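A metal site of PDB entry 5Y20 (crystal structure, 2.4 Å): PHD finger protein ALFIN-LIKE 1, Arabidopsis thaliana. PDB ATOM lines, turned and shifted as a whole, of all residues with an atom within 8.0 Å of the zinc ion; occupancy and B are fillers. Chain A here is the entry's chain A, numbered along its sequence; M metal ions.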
ATOM      1  N   CYS A  19      18.860   4.157  -4.939  1.00  0.00           N
ATOM      2  CA  CYS A  19      18.030   2.957  -4.902  1.00  0.00           C
ATOM      3  C   CYS A  19      17.254   2.814  -6.204  1.00  0.00           C
ATOM      4  O   CYS A  19      16.779   3.799  -6.765  1.00  0.00           O
ATOM      5  CB  CYS A  19      17.073   3.036  -3.713  1.00  0.00           C
ATOM      6  SG  CYS A  19      16.012   1.605  -3.411  1.00  0.00           S
ATOM      7  N   CYS A  20      17.104   1.580  -6.679  1.00  0.00           N
ATOM      8  CA  CYS A  20      16.349   1.331  -7.906  1.00  0.00           C
ATOM      9  C   CYS A  20      14.856   1.301  -7.602  1.00  0.00           C
ATOM     10  O   CYS A  20      14.411   0.584  -6.714  1.00  0.00           O
ATOM     11  CB  CYS A  20      16.792   0.013  -8.555  1.00  0.00           C
ATOM     12  SG  CYS A  20      15.860  -0.459 -10.052  1.00  0.00           S
ATOM     13  N   ASP A  21      14.086   2.091  -8.359  1.00  0.00           N
ATOM     14  CA  ASP A  21      12.643   2.179  -8.140  1.00  0.00           C
ATOM     15  C   ASP A  21      11.885   0.944  -8.623  1.00  0.00           C
ATOM     16  O   ASP A  21      10.717   0.779  -8.283  1.00  0.00           O
ATOM     17  CB  ASP A  21      12.091   3.427  -8.826  1.00  0.00           C
ATOM     18  CG  ASP A  21      12.516   4.704  -8.119  1.00  0.00           C
ATOM     19  OD1 ASP A  21      12.623   4.684  -6.881  1.00  0.00           O
ATOM     20  OD2 ASP A  21      12.728   5.726  -8.803  1.00  0.00           O
ATOM     21  N   VAL A  22      12.543   0.102  -9.416  1.00  0.00           N
ATOM     22  CA  VAL A  22      11.976  -1.154  -9.893  1.00  0.00           C
ATOM     23  C   VAL A  22      12.323  -2.358  -8.990  1.00  0.00           C
ATOM     24  O   VAL A  22      11.425  -2.989  -8.440  1.00  0.00           O
ATOM     25  CB  VAL A  22      12.453  -1.502 -11.329  1.00  0.00           C
ATOM     26  CG1 VAL A  22      11.697  -2.709 -11.853  1.00  0.00           C
ATOM     27  CG2 VAL A  22      12.271  -0.314 -12.250  1.00  0.00           C
ATOM     28  N   CYS A  23      13.618  -2.681  -8.845  1.00  0.00           N
ATOM     29  CA  CYS A  23      14.007  -3.856  -8.033  1.00  0.00           C
ATOM     30  C   CYS A  23      14.332  -3.524  -6.575  1.00  0.00           C
ATOM     31  O   CYS A  23      14.528  -4.437  -5.764  1.00  0.00           O
ATOM     32  CB  CYS A  23      15.212  -4.569  -8.660  1.00  0.00           C
ATOM     33  SG  CYS A  23      16.787  -3.689  -8.551  1.00  0.00           S
ATOM     34  N   GLU A  24      14.396  -2.231  -6.247  1.00  0.00           N
ATOM     35  CA  GLU A  24      14.685  -1.721  -4.898  1.00  0.00           C
ATOM     36  C   GLU A  24      15.993  -2.171  -4.259  1.00  0.00           C
ATOM     37  O   GLU A  24      16.132  -2.130  -3.039  1.00  0.00           O
ATOM     38  CB  GLU A  24      13.520  -2.051  -3.974  1.00  0.00           C
ATOM     39  CG  GLU A  24      12.317  -1.202  -4.303  1.00  0.00           C
ATOM     40  CD  GLU A  24      11.349  -1.105  -3.170  1.00  0.00           C
ATOM     41  OE1 GLU A  24      11.484  -1.903  -2.219  1.00  0.00           O
ATOM     42  OE2 GLU A  24      10.449  -0.248  -3.247  1.00  0.00           O
ATOM     43  N   ARG A  25      16.949  -2.579  -5.074  1.00  0.00           N
ATOM     44  CA  ARG A  25      18.298  -2.781  -4.560  1.00  0.00           C
ATOM     45  C   ARG A  25      18.923  -1.428  -4.298  1.00  0.00           C
ATOM     46  O   ARG A  25      18.642  -0.469  -5.009  1.00  0.00           O
ATOM     47  CB  ARG A  25      19.155  -3.582  -5.545  1.00  0.00           C
ATOM     48  CG  ARG A  25      18.828  -5.054  -5.653  1.00  0.00           C
ATOM     49  CD  ARG A  25      19.817  -5.733  -6.590  1.00  0.00           C
ATOM     50  NE  ARG A  25      19.465  -7.114  -6.855  1.00  0.00           N
ATOM     51  CZ  ARG A  25      18.672  -7.506  -7.853  1.00  0.00           C
ATOM     52  NH1 ARG A  25      18.393  -8.784  -8.031  1.00  0.00           N
ATOM     53  NH2 ARG A  25      18.166  -6.590  -8.683  1.00  0.00           N
ATOM     54  N   TRP A  26      19.775  -1.359  -3.286  1.00  0.00           N
ATOM     55  CA  TRP A  26      20.570  -0.169  -3.017  1.00  0.00           C
ATOM     56  C   TRP A  26      21.946  -0.286  -3.646  1.00  0.00           C
ATOM     57  O   TRP A  26      22.551  -1.357  -3.626  1.00  0.00           O
ATOM     58  CB  TRP A  26      20.683   0.079  -1.518  1.00  0.00           C
ATOM     59  CG  TRP A  26      19.532   0.867  -0.977  1.00  0.00           C
ATOM     60  CD1 TRP A  26      18.429   0.371  -0.312  1.00  0.00           C
ATOM     61  CD2 TRP A  26      19.346   2.278  -1.066  1.00  0.00           C
ATOM     62  NE1 TRP A  26      17.589   1.410   0.028  1.00  0.00           N
ATOM     63  CE2 TRP A  26      18.123   2.587  -0.427  1.00  0.00           C
ATOM     64  CE3 TRP A  26      20.098   3.328  -1.609  1.00  0.00           C
ATOM     65  CZ2 TRP A  26      17.653   3.882  -0.327  1.00  0.00           C
ATOM     66  CZ3 TRP A  26      19.619   4.613  -1.514  1.00  0.00           C
ATOM     67  CH2 TRP A  26      18.416   4.882  -0.873  1.00  0.00           C
ATOM     68  N   TYR A  27      22.452   0.817  -4.203  1.00  0.00           N
ATOM     69  CA  TYR A  27      23.725   0.803  -4.917  1.00  0.00           C
ATOM     70  C   TYR A  27      24.641   1.971  -4.536  1.00  0.00           C
ATOM     71  O   TYR A  27      24.149   3.055  -4.239  1.00  0.00           O
ATOM     72  CB  TYR A  27      23.506   0.880  -6.412  1.00  0.00           C
ATOM     73  CG  TYR A  27      22.797  -0.282  -7.067  1.00  0.00           C
ATOM     74  CD1 TYR A  27      23.503  -1.387  -7.501  1.00  0.00           C
ATOM     75  CD2 TYR A  27      21.424  -0.248  -7.306  1.00  0.00           C
ATOM     76  CE1 TYR A  27      22.862  -2.450  -8.131  1.00  0.00           C
ATOM     77  CE2 TYR A  27      20.786  -1.290  -7.943  1.00  0.00           C
ATOM     78  CZ  TYR A  27      21.510  -2.394  -8.352  1.00  0.00           C
ATOM     79  OH  TYR A  27      20.884  -3.440  -8.981  1.00  0.00           O
ATOM     80  N   TYR A  45      14.284   5.947 -11.046  1.00  0.00           N
ATOM     81  CA  TYR A  45      15.568   5.422 -11.443  1.00  0.00           C
ATOM     82  C   TYR A  45      15.473   3.936 -11.752  1.00  0.00           C
ATOM     83  O   TYR A  45      14.907   3.161 -10.978  1.00  0.00           O
ATOM     84  CB  TYR A  45      16.618   5.655 -10.342  1.00  0.00           C
ATOM     85  CG  TYR A  45      17.924   4.954 -10.647  1.00  0.00           C
ATOM     86  CD1 TYR A  45      18.674   5.315 -11.767  1.00  0.00           C
ATOM     87  CD2 TYR A  45      18.390   3.929  -9.850  1.00  0.00           C
ATOM     88  CE1 TYR A  45      19.853   4.679 -12.059  1.00  0.00           C
ATOM     89  CE2 TYR A  45      19.566   3.272 -10.136  1.00  0.00           C
ATOM     90  CZ  TYR A  45      20.297   3.654 -11.242  1.00  0.00           C
ATOM     91  OH  TYR A  45      21.480   3.009 -11.545  1.00  0.00           O
ATOM     92  N   LYS A  46      16.019   3.551 -12.896  1.00  0.00           N
ATOM     93  CA  LYS A  46      16.095   2.157 -13.288  1.00  0.00           C
ATOM     94  C   LYS A  46      17.561   1.709 -13.335  1.00  0.00           C
ATOM     95  O   LYS A  46      18.354   2.218 -14.121  1.00  0.00           O
ATOM     96  CB  LYS A  46      15.412   1.965 -14.637  1.00  0.00           C
ATOM     97  CG  LYS A  46      14.965   0.553 -14.933  1.00  0.00           C
ATOM     98  CD  LYS A  46      13.734   0.551 -15.854  1.00  0.00           C
ATOM     99  CE  LYS A  46      13.599  -0.796 -16.572  1.00  0.00           C
ATOM    100  NZ  LYS A  46      12.382  -0.875 -17.445  1.00  0.00           N
ATOM    101  N   CYS A  47      17.926   0.766 -12.462  1.00  0.00           N
ATOM    102  CA  CYS A  47      19.304   0.328 -12.354  1.00  0.00           C
ATOM    103  C   CYS A  47      19.715  -0.446 -13.608  1.00  0.00           C
ATOM    104  O   CYS A  47      18.850  -0.915 -14.346  1.00  0.00           O
ATOM    105  CB  CYS A  47      19.488  -0.520 -11.089  1.00  0.00           C
ATOM    106  SG  CYS A  47      19.016  -2.237 -11.219  1.00  0.00           S
ATOM    107  N   PRO A  48      21.028  -0.555 -13.881  1.00  0.00           N
ATOM    108  CA  PRO A  48      21.506  -1.183 -15.122  1.00  0.00           C
ATOM    109  C   PRO A  48      20.974  -2.596 -15.329  1.00  0.00           C
ATOM    110  O   PRO A  48      20.650  -2.994 -16.460  1.00  0.00           O
ATOM    111  CB  PRO A  48      23.024  -1.199 -14.935  1.00  0.00           C
ATOM    112  CG  PRO A  48      23.287  -0.025 -14.058  1.00  0.00           C
ATOM    113  CD  PRO A  48      22.150  -0.020 -13.087  1.00  0.00           C
ATOM    114  N   SER A  49      20.881  -3.341 -14.244  1.00  0.00           N
ATOM    115  CA  SER A  49      20.351  -4.695 -14.289  1.00  0.00           C
ATOM    116  C   SER A  49      18.885  -4.697 -14.714  1.00  0.00           C
ATOM    117  O   SER A  49      18.456  -5.574 -15.468  1.00  0.00           O
ATOM    118  CB  SER A  49      20.516  -5.362 -12.930  1.00  0.00           C
ATOM    119  OG  SER A  49      19.750  -6.541 -12.846  1.00  0.00           O
ATOM    120  N   CYS A  50      18.129  -3.714 -14.250  1.00  0.00           N
ATOM    121  CA  CYS A  50      16.708  -3.637 -14.570  1.00  0.00           C
ATOM    122  C   CYS A  50      16.459  -3.139 -16.007  1.00  0.00           C
ATOM    123  O   CYS A  50      15.422  -3.439 -16.596  1.00  0.00           O
ATOM    124  CB  CYS A  50      15.979  -2.728 -13.565  1.00  0.00           C
ATOM    125  SG  CYS A  50      15.543  -3.556 -12.009  1.00  0.00           S
ATOM    126  N   CYS A  51      17.410  -2.401 -16.584  1.00  0.00           N
ATOM    127  CA  CYS A  51      17.318  -2.036 -17.995  1.00  0.00           C
ATOM    128  C   CYS A  51      17.554  -3.237 -18.912  1.00  0.00           C
ATOM    129  O   CYS A  51      17.525  -3.104 -20.134  1.00  0.00           O
ATOM    130  CB  CYS A  51      18.318  -0.937 -18.330  1.00  0.00           C
ATOM    131  SG  CYS A  51      17.920   0.651 -17.613  1.00  0.00           S
HETATM  132 ZN    ZN M   1      16.828  -2.506 -10.438  1.00  0.00          ZN
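The zinc ion is bound by SG of Cys 23 (2.2 Å), SG of Cys 50 (2.3 Å), SG of Cys 20 (2.3 Å) and SG of Cys 47 (2.3 Å).
The side-chain sulfur of Cys 23 sits close to the guanidinium group of Arg 25, 3.2 Å away. The backbone NH (N) of Val 22 sits close to the side-chain sulfur (SG) of Cys 20, 3.4 Å away. The backbone carbonyl oxygen of Arg 25 is in hydrogen-bond range of the backbone NH of Cys 20 (3.1 Å). OH of Tyr 27 sits close to SG of Cys 47, at 3.2 Å. SG of Cys 47 lies close to N of Ser 49 (3.7 Å). O of Cys 47 lies within hydrogen-bond range of SG of Cys 51 (3.7 Å).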
